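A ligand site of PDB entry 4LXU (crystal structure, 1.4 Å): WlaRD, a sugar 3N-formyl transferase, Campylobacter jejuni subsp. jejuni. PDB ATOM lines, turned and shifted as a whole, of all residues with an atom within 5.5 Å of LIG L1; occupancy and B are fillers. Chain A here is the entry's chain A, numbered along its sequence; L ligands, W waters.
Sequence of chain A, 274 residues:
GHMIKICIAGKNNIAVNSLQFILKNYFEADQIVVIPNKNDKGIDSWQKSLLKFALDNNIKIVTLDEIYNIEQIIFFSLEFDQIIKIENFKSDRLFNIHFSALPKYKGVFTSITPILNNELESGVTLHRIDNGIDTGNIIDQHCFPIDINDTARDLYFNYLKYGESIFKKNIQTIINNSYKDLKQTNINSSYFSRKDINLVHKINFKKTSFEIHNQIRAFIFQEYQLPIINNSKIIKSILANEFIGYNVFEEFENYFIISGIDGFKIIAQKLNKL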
ATOM      1  N   LYS A  11     -25.064   5.608  -6.197  1.00  0.00           N
ATOM      2  CA  LYS A  11     -26.302   4.841  -6.445  1.00  0.00           C
ATOM      3  C   LYS A  11     -26.199   3.428  -5.953  1.00  0.00           C
ATOM      4  O   LYS A  11     -25.138   2.919  -5.572  1.00  0.00           O
ATOM      5  CB  LYS A  11     -26.640   4.817  -7.962  1.00  0.00           C
ATOM      6  CG  LYS A  11     -25.667   3.942  -8.782  1.00  0.00           C
ATOM      7  CD  LYS A  11     -26.234   3.777 -10.200  1.00  0.00           C
ATOM      8  CE  LYS A  11     -25.183   3.051 -11.002  1.00  0.00           C
ATOM      9  NZ  LYS A  11     -25.674   2.869 -12.450  1.00  0.00           N
ATOM     10  N   ASN A  12     -27.380   2.797  -6.022  1.00  0.00           N
ATOM     11  CA  ASN A  12     -27.549   1.338  -5.836  1.00  0.00           C
ATOM     12  C   ASN A  12     -27.339   0.866  -4.406  1.00  0.00           C
ATOM     13  O   ASN A  12     -27.213   1.740  -3.530  1.00  0.00           O
ATOM     14  CB  ASN A  12     -26.729   0.532  -6.877  1.00  0.00           C
ATOM     15  CG  ASN A  12     -27.296   0.692  -8.272  1.00  0.00           C
ATOM     16  OD1 ASN A  12     -28.364   1.298  -8.465  1.00  0.00           O
ATOM     17  ND2 ASN A  12     -26.586   0.156  -9.255  1.00  0.00           N
ATOM     18  N   ASN A  37     -27.097   9.884  -8.579  1.00  0.00           N
ATOM     19  CA  ASN A  37     -26.755   9.884 -10.015  1.00  0.00           C
ATOM     20  C   ASN A  37     -27.892  10.492 -10.828  1.00  0.00           C
ATOM     21  O   ASN A  37     -29.037  10.583 -10.391  1.00  0.00           O
ATOM     22  CB  ASN A  37     -26.441   8.471 -10.494  1.00  0.00           C
ATOM     23  CG  ASN A  37     -25.061   8.040 -10.058  1.00  0.00           C
ATOM     24  OD1 ASN A  37     -24.363   8.759  -9.322  1.00  0.00           O
ATOM     25  ND2 ASN A  37     -24.612   6.903 -10.504  1.00  0.00           N
ATOM     26  N   GLU A  79     -20.284   4.378  -6.616  1.00  0.00           N
ATOM     27  CA  GLU A  79     -20.864   4.304  -7.956  1.00  0.00           C
ATOM     28  C   GLU A  79     -21.373   5.625  -8.481  1.00  0.00           C
ATOM     29  O   GLU A  79     -22.305   5.698  -9.296  1.00  0.00           O
ATOM     30  CB  GLU A  79     -21.928   3.179  -8.071  1.00  0.00           C
ATOM     31  CG  GLU A  79     -21.349   1.777  -7.840  1.00  0.00           C
ATOM     32  CD  GLU A  79     -20.076   1.567  -8.684  1.00  0.00           C
ATOM     33  OE1 GLU A  79     -20.155   1.341  -9.940  1.00  0.00           O
ATOM     34  OE2 GLU A  79     -18.917   1.558  -8.155  1.00  0.00           O
ATOM     35  N   PHE A  80     -20.731   6.725  -8.081  1.00  0.00           N
ATOM     36  CA  PHE A  80     -21.074   8.033  -8.616  1.00  0.00           C
ATOM     37  C   PHE A  80     -20.724   8.178 -10.094  1.00  0.00           C
ATOM     38  O   PHE A  80     -19.697   7.669 -10.555  1.00  0.00           O
ATOM     39  CB  PHE A  80     -20.361   9.131  -7.765  1.00  0.00           C
ATOM     40  CG  PHE A  80     -20.760  10.541  -8.010  1.00  0.00           C
ATOM     41  CD1 PHE A  80     -19.776  11.547  -8.127  1.00  0.00           C
ATOM     42  CD2 PHE A  80     -22.099  10.890  -8.068  1.00  0.00           C
ATOM     43  CE1 PHE A  80     -20.163  12.889  -8.273  1.00  0.00           C
ATOM     44  CE2 PHE A  80     -22.505  12.217  -8.234  1.00  0.00           C
ATOM     45  CZ  PHE A  80     -21.529  13.226  -8.295  1.00  0.00           C
ATOM     46  N   ASP A  81     -21.583   8.911 -10.781  1.00  0.00           N
ATOM     47  CA  ASP A  81     -21.533   9.016 -12.246  1.00  0.00           C
ATOM     48  C   ASP A  81     -20.740  10.179 -12.810  1.00  0.00           C
ATOM     49  O   ASP A  81     -20.565  10.294 -14.026  1.00  0.00           O
ATOM     50  CB  ASP A  81     -22.923   8.970 -12.905  1.00  0.00           C
ATOM     51  CG  ASP A  81     -23.820  10.092 -12.466  1.00  0.00           C
ATOM     52  OD1 ASP A  81     -24.934  10.212 -13.046  1.00  0.00           O
ATOM     53  OD2 ASP A  81     -23.465  10.936 -11.594  1.00  0.00           O
ATOM     54  N   GLN A  82     -20.314  11.093 -11.946  1.00  0.00           N
ATOM     55  CA  GLN A  82     -19.584  12.289 -12.416  1.00  0.00           C
ATOM     56  C   GLN A  82     -18.117  12.271 -12.062  1.00  0.00           C
ATOM     57  O   GLN A  82     -17.777  11.998 -10.913  1.00  0.00           O
ATOM     58  CB  GLN A  82     -20.181  13.584 -11.867  1.00  0.00           C
ATOM     59  CG  GLN A  82     -21.659  13.825 -12.153  1.00  0.00           C
ATOM     60  CD  GLN A  82     -22.139  15.209 -11.705  1.00  0.00           C
ATOM     61  OE1 GLN A  82     -21.619  16.189 -12.254  1.00  0.00           O
ATOM     62  NE2 GLN A  82     -23.090  15.299 -10.772  1.00  0.00           N
ATOM     63  N   ASN A  96     -13.375   7.019  -3.088  1.00  0.00           N
ATOM     64  CA  ASN A  96     -14.212   6.187  -3.985  1.00  0.00           C
ATOM     65  C   ASN A  96     -13.939   4.738  -3.645  1.00  0.00           C
ATOM     66  O   ASN A  96     -12.836   4.350  -3.236  1.00  0.00           O
ATOM     67  CB  ASN A  96     -13.827   6.470  -5.448  1.00  0.00           C
ATOM     68  CG  ASN A  96     -14.588   5.596  -6.434  1.00  0.00           C
ATOM     69  OD1 ASN A  96     -13.939   4.722  -7.115  1.00  0.00           O
ATOM     70  ND2 ASN A  96     -15.865   5.780  -6.538  1.00  0.00           N
ATOM     71  N   HIS A  98     -13.879   1.496  -5.996  1.00  0.00           N
ATOM     72  CA  HIS A  98     -13.832   1.034  -7.382  1.00  0.00           C
ATOM     73  C   HIS A  98     -14.054  -0.456  -7.446  1.00  0.00           C
ATOM     74  O   HIS A  98     -13.447  -1.235  -6.731  1.00  0.00           O
ATOM     75  CB  HIS A  98     -12.506   1.424  -8.043  1.00  0.00           C
ATOM     76  CG  HIS A  98     -12.474   0.998  -9.492  1.00  0.00           C
ATOM     77  ND1 HIS A  98     -13.243   1.623 -10.456  1.00  0.00           N
ATOM     78  CD2 HIS A  98     -11.787   0.016 -10.112  1.00  0.00           C
ATOM     79  CE1 HIS A  98     -13.026   1.027 -11.632  1.00  0.00           C
ATOM     80  NE2 HIS A  98     -12.137   0.069 -11.444  1.00  0.00           N
ATOM     81  N   GLY A 107     -11.769   2.390 -15.176  1.00  0.00           N
ATOM     82  CA  GLY A 107     -12.748   2.800 -16.168  1.00  0.00           C
ATOM     83  C   GLY A 107     -14.113   2.198 -15.865  1.00  0.00           C
ATOM     84  O   GLY A 107     -14.571   2.261 -14.717  1.00  0.00           O
ATOM     85  N   VAL A 108     -14.797   1.707 -16.890  1.00  0.00           N
ATOM     86  CA  VAL A 108     -16.223   1.371 -16.799  1.00  0.00           C
ATOM     87  C   VAL A 108     -16.441  -0.094 -17.184  1.00  0.00           C
ATOM     88  O   VAL A 108     -15.498  -0.823 -17.537  1.00  0.00           O
ATOM     89  CB  VAL A 108     -17.051   2.305 -17.678  1.00  0.00           C
ATOM     90  CG1 VAL A 108     -16.815   3.807 -17.226  1.00  0.00           C
ATOM     91  CG2 VAL A 108     -16.747   2.065 -19.127  1.00  0.00           C
ATOM     92  N   PHE A 109     -17.692  -0.497 -16.994  1.00  0.00           N
ATOM     93  CA  PHE A 109     -18.073  -1.894 -17.396  1.00  0.00           C
ATOM     94  C   PHE A 109     -17.243  -2.928 -16.677  1.00  0.00           C
ATOM     95  O   PHE A 109     -16.873  -3.973 -17.252  1.00  0.00           O
ATOM     96  CB  PHE A 109     -18.067  -2.124 -18.926  1.00  0.00           C
ATOM     97  CG  PHE A 109     -19.066  -1.340 -19.696  1.00  0.00           C
ATOM     98  CD1 PHE A 109     -18.727  -0.755 -20.886  1.00  0.00           C
ATOM     99  CD2 PHE A 109     -20.353  -1.182 -19.229  1.00  0.00           C
ATOM    100  CE1 PHE A 109     -19.645  -0.035 -21.666  1.00  0.00           C
ATOM    101  CE2 PHE A 109     -21.296  -0.444 -19.981  1.00  0.00           C
ATOM    102  CZ  PHE A 109     -20.949   0.109 -21.221  1.00  0.00           C
ATOM    103  N   THR A 110     -16.960  -2.736 -15.392  1.00  0.00           N
ATOM    104  CA  THR A 110     -16.027  -3.621 -14.738  1.00  0.00           C
ATOM    105  C   THR A 110     -16.606  -4.965 -14.285  1.00  0.00           C
ATOM    106  O   THR A 110     -15.865  -5.792 -13.767  1.00  0.00           O
ATOM    107  CB  THR A 110     -15.338  -2.931 -13.533  1.00  0.00           C
ATOM    108  OG1 THR A 110     -16.317  -2.741 -12.526  1.00  0.00           O
ATOM    109  CG2 THR A 110     -14.649  -1.601 -13.836  1.00  0.00           C
ATOM    110  N   SER A 111     -17.904  -5.181 -14.507  1.00  0.00           N
ATOM    111  CA  SER A 111     -18.475  -6.507 -14.402  1.00  0.00           C
ATOM    112  C   SER A 111     -18.301  -7.285 -15.693  1.00  0.00           C
ATOM    113  O   SER A 111     -18.538  -8.512 -15.654  1.00  0.00           O
ATOM    114  CB  SER A 111     -19.945  -6.431 -13.977  1.00  0.00           C
ATOM    115  OG  SER A 111     -20.077  -5.809 -12.693  1.00  0.00           O
ATOM    116  N   ILE A 112     -17.957  -6.603 -16.782  1.00  0.00           N
ATOM    117  CA  ILE A 112     -17.743  -7.269 -18.080  1.00  0.00           C
ATOM    118  C   ILE A 112     -16.241  -7.467 -18.331  1.00  0.00           C
ATOM    119  O   ILE A 112     -15.774  -8.570 -18.643  1.00  0.00           O
ATOM    120  CB  ILE A 112     -18.350  -6.405 -19.205  1.00  0.00           C
ATOM    121  CG1 ILE A 112     -19.871  -6.214 -18.977  1.00  0.00           C
ATOM    122  CG2 ILE A 112     -18.023  -7.037 -20.614  1.00  0.00           C
ATOM    123  CD1 ILE A 112     -20.551  -5.404 -20.070  1.00  0.00           C
ATOM    124  N   ASP A 134      -9.930   6.461 -11.582  1.00  0.00           N
ATOM    125  CA  ASP A 134      -9.561   5.329 -10.748  1.00  0.00           C
ATOM    126  C   ASP A 134      -8.060   5.178 -10.555  1.00  0.00           C
ATOM    127  O   ASP A 134      -7.545   4.085 -10.364  1.00  0.00           O
ATOM    128  CB  ASP A 134     -10.120   3.997 -11.338  1.00  0.00           C
ATOM    129  CG  ASP A 134     -11.595   4.078 -11.650  1.00  0.00           C
ATOM    130  OD1 ASP A 134     -12.378   4.643 -10.838  1.00  0.00           O
ATOM    131  OD2 ASP A 134     -12.006   3.571 -12.743  1.00  0.00           O
ATOM    132  N   ALA A 152     -21.640 -11.744 -15.625  1.00  0.00           N
ATOM    133  CA  ALA A 152     -21.410 -10.310 -15.282  1.00  0.00           C
ATOM    134  C   ALA A 152     -22.353  -9.871 -14.183  1.00  0.00           C
ATOM    135  O   ALA A 152     -21.930  -9.135 -13.246  1.00  0.00           O
ATOM    136  CB  ALA A 152     -21.624  -9.490 -16.510  1.00  0.00           C
ATOM    137  N   TYR A 156     -21.275  -8.415 -10.570  1.00  0.00           N
ATOM    138  CA  TYR A 156     -21.745  -7.121 -10.070  1.00  0.00           C
ATOM    139  C   TYR A 156     -22.333  -7.238  -8.683  1.00  0.00           C
ATOM    140  O   TYR A 156     -22.064  -6.404  -7.807  1.00  0.00           O
ATOM    141  CB  TYR A 156     -22.782  -6.472 -11.011  1.00  0.00           C
ATOM    142  CG  TYR A 156     -23.126  -5.042 -10.629  1.00  0.00           C
ATOM    143  CD1 TYR A 156     -22.195  -4.017 -10.838  1.00  0.00           C
ATOM    144  CD2 TYR A 156     -24.348  -4.740 -10.042  1.00  0.00           C
ATOM    145  CE1 TYR A 156     -22.494  -2.689 -10.455  1.00  0.00           C
ATOM    146  CE2 TYR A 156     -24.649  -3.430  -9.691  1.00  0.00           C
ATOM    147  CZ  TYR A 156     -23.719  -2.451  -9.875  1.00  0.00           C
ATOM    148  OH  TYR A 156     -24.034  -1.159  -9.470  1.00  0.00           O
ATOM    149  N   ARG A 194     -16.262   3.333 -22.366  1.00  0.00           N
ATOM    150  CA  ARG A 194     -17.513   2.812 -22.911  1.00  0.00           C
ATOM    151  C   ARG A 194     -17.303   2.407 -24.362  1.00  0.00           C
ATOM    152  O   ARG A 194     -17.810   1.365 -24.780  1.00  0.00           O
ATOM    153  CB  ARG A 194     -18.674   3.792 -22.709  1.00  0.00           C
ATOM    154  CG  ARG A 194     -18.978   4.248 -21.261  1.00  0.00           C
ATOM    155  CD  ARG A 194     -19.954   3.347 -20.463  1.00  0.00           C
ATOM    156  NE  ARG A 194     -20.329   3.825 -19.134  1.00  0.00           N
ATOM    157  CZ  ARG A 194     -20.721   3.047 -18.139  1.00  0.00           C
ATOM    158  NH1 ARG A 194     -21.036   3.552 -16.954  1.00  0.00           N
ATOM    159  NH2 ARG A 194     -20.875   1.731 -18.338  1.00  0.00           N
ATOM    160  N   LEU A 199     -21.842  -3.562 -26.566  1.00  0.00           N
ATOM    161  CA  LEU A 199     -22.723  -4.284 -25.667  1.00  0.00           C
ATOM    162  C   LEU A 199     -23.563  -5.338 -26.378  1.00  0.00           C
ATOM    163  O   LEU A 199     -24.212  -6.135 -25.707  1.00  0.00           O
ATOM    164  CB  LEU A 199     -23.623  -3.306 -24.891  1.00  0.00           C
ATOM    165  CG  LEU A 199     -22.832  -2.530 -23.841  1.00  0.00           C
ATOM    166  CD1 LEU A 199     -23.656  -1.286 -23.450  1.00  0.00           C
ATOM    167  CD2 LEU A 199     -22.388  -3.332 -22.629  1.00  0.00           C
ATOM    168  N   PHE A 219     -21.408 -11.004 -20.892  1.00  0.00           N
ATOM    169  CA  PHE A 219     -22.501 -10.183 -21.339  1.00  0.00           C
ATOM    170  C   PHE A 219     -23.870 -10.589 -20.783  1.00  0.00           C
ATOM    171  O   PHE A 219     -24.885  -9.985 -21.108  1.00  0.00           O
ATOM    172  CB  PHE A 219     -22.513 -10.065 -22.875  1.00  0.00           C
ATOM    173  CG  PHE A 219     -21.363  -9.279 -23.392  1.00  0.00           C
ATOM    174  CD1 PHE A 219     -21.426  -7.878 -23.471  1.00  0.00           C
ATOM    175  CD2 PHE A 219     -20.157  -9.896 -23.707  1.00  0.00           C
ATOM    176  CE1 PHE A 219     -20.328  -7.145 -23.947  1.00  0.00           C
ATOM    177  CE2 PHE A 219     -19.062  -9.178 -24.164  1.00  0.00           C
ATOM    178  CZ  PHE A 219     -19.157  -7.773 -24.270  1.00  0.00           C
ATOM    179  N   PHE A 221     -26.299 -10.121 -18.354  1.00  0.00           N
ATOM    180  CA  PHE A 221     -26.738  -9.227 -17.260  1.00  0.00           C
ATOM    181  C   PHE A 221     -28.133  -8.781 -17.635  1.00  0.00           C
ATOM    182  O   PHE A 221     -28.304  -7.761 -18.260  1.00  0.00           O
ATOM    183  CB  PHE A 221     -25.743  -8.052 -17.064  1.00  0.00           C
ATOM    184  CG  PHE A 221     -25.839  -7.348 -15.700  1.00  0.00           C
ATOM    185  CD1 PHE A 221     -24.649  -6.887 -15.104  1.00  0.00           C
ATOM    186  CD2 PHE A 221     -27.038  -7.103 -15.051  1.00  0.00           C
ATOM    187  CE1 PHE A 221     -24.727  -6.183 -13.869  1.00  0.00           C
ATOM    188  CE2 PHE A 221     -27.090  -6.414 -13.794  1.00  0.00           C
ATOM    189  CZ  PHE A 221     -25.894  -5.963 -13.240  1.00  0.00           C
ATOM    190  N   TYR A 224     -29.931  -5.515 -18.343  1.00  0.00           N
ATOM    191  CA  TYR A 224     -29.418  -4.733 -19.447  1.00  0.00           C
ATOM    192  C   TYR A 224     -29.486  -5.496 -20.798  1.00  0.00           C
ATOM    193  O   TYR A 224     -30.107  -4.955 -21.728  1.00  0.00           O
ATOM    194  CB  TYR A 224     -27.964  -4.345 -19.157  1.00  0.00           C
ATOM    195  CG  TYR A 224     -27.809  -3.379 -17.991  1.00  0.00           C
ATOM    196  CD1 TYR A 224     -28.206  -2.052 -18.113  1.00  0.00           C
ATOM    197  CD2 TYR A 224     -27.308  -3.829 -16.769  1.00  0.00           C
ATOM    198  CE1 TYR A 224     -28.055  -1.154 -17.055  1.00  0.00           C
ATOM    199  CE2 TYR A 224     -27.166  -2.926 -15.692  1.00  0.00           C
ATOM    200  CZ  TYR A 224     -27.548  -1.633 -15.869  1.00  0.00           C
ATOM    201  OH  TYR A 224     -27.361  -0.764 -14.807  1.00  0.00           O
ATOM    202  N   GLN A 225     -28.816  -6.642 -20.910  1.00  0.00           N
ATOM    203  CA  GLN A 225     -28.886  -7.391 -22.199  1.00  0.00           C
ATOM    204  C   GLN A 225     -28.476  -8.791 -21.874  1.00  0.00           C
ATOM    205  O   GLN A 225     -27.945  -9.134 -20.806  1.00  0.00           O
ATOM    206  CB  GLN A 225     -27.969  -6.795 -23.275  1.00  0.00           C
ATOM    207  CG  GLN A 225     -26.457  -7.031 -23.096  1.00  0.00           C
ATOM    208  CD  GLN A 225     -25.857  -6.233 -21.952  1.00  0.00           C
ATOM    209  OE1 GLN A 225     -25.950  -5.009 -21.912  1.00  0.00           O
ATOM    210  NE2 GLN A 225     -25.248  -6.974 -21.041  1.00  0.00           N
HETATM  211  O1  LIG L   1     -19.665  -0.814 -14.002  1.00  0.00           O
HETATM  212  P1  LIG L   1     -20.072   0.474 -14.535  1.00  0.00           P
HETATM  213  O2  LIG L   1     -20.002   0.838 -15.951  1.00  0.00           O
HETATM  214  O3  LIG L   1     -19.155   1.536 -13.705  1.00  0.00           O
HETATM  215  C1  LIG L   1     -19.056   2.891 -14.147  1.00  0.00           C
HETATM  216  O4  LIG L   1     -20.229   3.659 -14.012  1.00  0.00           O
HETATM  217  C2  LIG L   1     -20.666   3.794 -12.651  1.00  0.00           C
HETATM  218  C3  LIG L   1     -21.981   4.529 -12.733  1.00  0.00           C
HETATM  219  C4  LIG L   1     -17.914   3.537 -13.339  1.00  0.00           C
HETATM  220  O5  LIG L   1     -16.847   2.581 -13.318  1.00  0.00           O
HETATM  221  C5  LIG L   1     -18.309   3.795 -11.900  1.00  0.00           C
HETATM  222  N1  LIG L   1     -17.246   4.637 -11.260  1.00  0.00           N
HETATM  223  C6  LIG L   1     -19.604   4.614 -11.889  1.00  0.00           C
HETATM  224  O6  LIG L   1     -19.423   5.898 -12.494  1.00  0.00           O
HETATM  225  O7  LIG L   1     -21.493   0.816 -13.904  1.00  0.00           O
HETATM  226  P2  LIG L   1     -23.008   0.763 -14.424  1.00  0.00           P
HETATM  227  O8  LIG L   1     -23.807   0.985 -13.164  1.00  0.00           O
HETATM  228  O9  LIG L   1     -23.361   1.612 -15.576  1.00  0.00           O
HETATM  229  O10 LIG L   1     -23.167  -0.765 -14.903  1.00  0.00           O
HETATM  230  C7  LIG L   1     -22.927  -1.792 -13.928  1.00  0.00           C
HETATM  231  C8  LIG L   1     -22.670  -3.092 -14.662  1.00  0.00           C
HETATM  232  O11 LIG L   1     -23.858  -3.428 -15.420  1.00  0.00           O
HETATM  233  C9  LIG L   1     -21.554  -2.942 -15.668  1.00  0.00           C
HETATM  234  O12 LIG L   1     -20.256  -3.218 -15.143  1.00  0.00           O
HETATM  235  C10 LIG L   1     -21.907  -4.106 -16.630  1.00  0.00           C
HETATM  236  C11 LIG L   1     -23.422  -4.014 -16.642  1.00  0.00           C
HETATM  237  N2  LIG L   1     -24.015  -3.306 -17.778  1.00  0.00           N
HETATM  238  C12 LIG L   1     -24.409  -3.983 -18.894  1.00  0.00           C
HETATM  239  O13 LIG L   1     -24.152  -5.187 -18.939  1.00  0.00           O
HETATM  240  N3  LIG L   1     -24.979  -3.321 -19.920  1.00  0.00           N
HETATM  241  C13 LIG L   1     -24.240  -1.987 -17.683  1.00  0.00           C
HETATM  242  C14 LIG L   1     -24.856  -1.272 -18.699  1.00  0.00           C
HETATM  243  C15 LIG L   1     -25.097   0.227 -18.584  1.00  0.00           C
HETATM  244  C16 LIG L   1     -25.246  -2.013 -19.828  1.00  0.00           C
HETATM  245  O14 LIG L   1     -25.869  -1.425 -20.858  1.00  0.00           O
HETATM  246  N1  LG2 L   2     -13.747  11.552 -10.173  1.00  0.00           N
HETATM  247  C1  LG2 L   2     -12.438  11.375 -10.419  1.00  0.00           C
HETATM  248  N2  LG2 L   2     -11.681  12.474 -10.744  1.00  0.00           N
HETATM  249  N3  LG2 L   2     -11.772  10.217 -10.331  1.00  0.00           N
HETATM  250  C2  LG2 L   2     -12.490   9.109 -10.086  1.00  0.00           C
HETATM  251  O1  LG2 L   2     -11.712   8.025  -9.949  1.00  0.00           O
HETATM  252  C3  LG2 L   2     -13.852   9.184  -9.837  1.00  0.00           C
HETATM  253  N4  LG2 L   2     -14.694   8.031  -9.731  1.00  0.00           N
HETATM  254  C4  LG2 L   2     -16.123   8.296 -10.008  1.00  0.00           C
HETATM  255  C5  LG2 L   2     -16.566   9.511  -9.198  1.00  0.00           C
HETATM  256  N5  LG2 L   2     -15.761  10.666  -9.626  1.00  0.00           N
HETATM  257  C6  LG2 L   2     -14.461  10.440  -9.905  1.00  0.00           C
HETATM  258  C7  LG2 L   2     -16.588   8.536 -11.453  1.00  0.00           C
HETATM  259  N6  LG2 L   2     -16.320   7.371 -12.307  1.00  0.00           N
HETATM  260  C8  LG2 L   2     -16.850   7.945 -16.427  1.00  0.00           C
HETATM  261  C9  LG2 L   2     -17.602   8.670 -15.511  1.00  0.00           C
HETATM  262  C10 LG2 L   2     -17.446   8.495 -14.125  1.00  0.00           C
HETATM  263  C11 LG2 L   2     -16.513   7.591 -13.635  1.00  0.00           C
HETATM  264  C12 LG2 L   2     -15.781   6.825 -14.552  1.00  0.00           C
HETATM  265  C13 LG2 L   2     -15.919   7.034 -15.922  1.00  0.00           C
HETATM  266  C14 LG2 L   2     -16.985   8.194 -17.887  1.00  0.00           C
HETATM  267  O2  LG2 L   2     -17.881   8.916 -18.283  1.00  0.00           O
HETATM  268  N7  LG2 L   2     -16.089   7.659 -18.705  1.00  0.00           N
HETATM  269  C15 LG2 L   2     -16.105   7.944 -20.150  1.00  0.00           C
HETATM  270  C16 LG2 L   2     -14.722   8.518 -20.525  1.00  0.00           C
HETATM  271  C17 LG2 L   2     -14.523   9.931 -19.931  1.00  0.00           C
HETATM  272  C18 LG2 L   2     -13.245  10.585 -20.399  1.00  0.00           C
HETATM  273  O3  LG2 L   2     -12.502  10.041 -21.250  1.00  0.00           O
HETATM  274  O4  LG2 L   2     -12.990  11.712 -19.882  1.00  0.00           O
HETATM  275  C19 LG2 L   2     -16.299   6.715 -21.000  1.00  0.00           C
HETATM  276  O5  LG2 L   2     -15.918   5.623 -20.549  1.00  0.00           O
HETATM  277  O6  LG2 L   2     -16.840   6.903 -22.113  1.00  0.00           O
HETATM  278  C20 LG2 L   2     -14.321   6.803  -9.666  1.00  0.00           C
HETATM  279  O7  LG2 L   2     -15.196   5.899  -9.765  1.00  0.00           O
HETATM  280  O   HOH W   1     -17.593   4.278  -8.305  1.00  0.00           O
HETATM  281  O   HOH W   2     -14.983   3.300  -9.453  1.00  0.00           O
HETATM  282  O   HOH W   3     -19.177  -0.573 -11.556  1.00  0.00           O
HETATM  283  O   HOH W   4     -16.842   0.277 -12.086  1.00  0.00           O
HETATM  284  O   HOH W   5     -24.907   3.414 -16.002  1.00  0.00           O
HETATM  285  O   HOH W   6     -26.234  -0.312 -12.228  1.00  0.00           O
HETATM  286  O   HOH W   7     -19.093  -3.178 -12.230  1.00  0.00           O
HETATM  287  O   HOH W   8     -26.069   1.038 -21.898  1.00  0.00           O
HETATM  288  O   HOH W   9     -14.604   4.376 -12.469  1.00  0.00           O
HETATM  289  O   HOH W  10     -20.490   6.679 -15.336  1.00  0.00           O
HETATM  290  O   HOH W  11     -22.665   0.747 -10.671  1.00  0.00           O
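The backbone carbonyl oxygen (O) of Phe 80 is in hydrogen-bond range of an oxygen (O6) of LIG L1 (2.6 Å).
The backbone carbonyl oxygen (O) of Gly 107 is in hydrogen-bond range of an oxygen (O5) of LIG L1 (2.7 Å).
The guanidinium group of Arg 194 is in salt-bridge range of an oxygen (O2) of LIG L1, at 2.7 Å.
An oxygen (O8) of LIG L1 lies within salt-bridge range of the side-chain amino group of Lys 11, 2.7 Å away.
A nitrogen (N3) of LIG L1 lies within hydrogen-bond range of the side-chain amide oxygen (OE1) of Gln 225, at 2.8 Å.
An oxygen (O2) of LIG L1 lies within hydrogen-bond range of the backbone NH (N) of Phe 109, at 2.9 Å.
N of Ser 111 is in hydrogen-bond range of O12 of LIG L1 (3.1 Å).
The backbone NH of Thr 110 sits at hydrogen-bond distance from an oxygen (O12) of LIG L1 (3.3 Å).
An oxygen (O5) of LG2 L2 is in hydrogen-bond range of the backbone NH (N) of Arg 194 (2.9 Å).
The backbone NH (N) of Asp 134 lies within hydrogen-bond range of an oxygen (O1) of LG2 L2 (2.9 Å).
An oxygen (O7) of LG2 L2 sits close to the side-chain amide oxygen (OD1) of Asn 96.
The backbone carbonyl oxygen of Gln 82 is in hydrogen-bond range of a nitrogen (N5) of LG2 L2 (2.7 Å).
OD2 of Asp 134 lies within hydrogen-bond range of N of Gly 107 (2.7 Å).
O of Phe 219 lies within hydrogen-bond range of NE2 of Gln 225 (3.0 Å).
The side-chain hydroxyl (OH) of Tyr 156 sits at hydrogen-bond distance from the side-chain amide nitrogen (ND2) of Asn 12 (2.9 Å).
The backbone carbonyl oxygen (O) of Glu 79 lies within hydrogen-bond range of the side-chain amide nitrogen (ND2) of Asn 37.
The backbone NH (N) of Asp 81 lies within hydrogen-bond range of the side-chain amide oxygen (OD1) of Asn 37.
An oxygen (O7) of LG2 L2 lies within hydrogen-bond range of a nitrogen (N1) of LIG L1 (2.8 Å).
Residues that only touch LIG L1: Tyr 224 (3.2 Å), Phe 221 (3.3 Å), Leu 199 (3.4 Å), Tyr 156 (3.6 Å), Glu 79 (3.6 Å), Val 108 (3.7 Å), Ile 112 (3.8 Å) and Asp 81 (3.8 Å).
Within 4 Å of LIG L1: Lys 11, Glu 79, Phe 80, Asp 81, Gly 107, Val 108, Phe 109, Thr 110, Ser 111, Ile 112, Tyr 156, Arg 194, Leu 199, Phe 221, Tyr 224 and Gln 225.
Water W3 lies within hydrogen-bond range of O1 of LIG L1 (2.5 Å) and OE1 of Glu 79 (2.7 Å).
Water W4 bridges O5 of LIG L1 (2.6 Å) and OG1 of Thr 110 (3.1 Å).
Water W11 lies within hydrogen-bond range of the side-chain hydroxyl (OH) of Tyr 156, the side-chain carboxylate (OE1) of Glu 79 and an oxygen (O8) of LIG L1.
Water W6 lies within hydrogen-bond range of the side-chain hydroxyl (OH) of Tyr 224 (2.9 Å), an oxygen (O8) of LIG L1 (2.9 Å), the side-chain amide nitrogen (ND2) of Asn 12 (3.0 Å) and the side-chain amino group (NZ) of Lys 11 (3.2 Å).
Water W1 lies within hydrogen-bond range of the side-chain amide nitrogen (ND2) of Asn 96 (2.9 Å), a nitrogen (N1) of LIG L1 (3.0 Å), the side-chain carboxylate (OE2) of Glu 79 (3.0 Å) and an oxygen (O7) of LG2 L2 (3.2 Å).
Water W7 lies within hydrogen-bond range of the side-chain hydroxyl (OG1) of Thr 110, the side-chain hydroxyl (OG) of Ser 111 and an oxygen (O1) of LIG L1.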
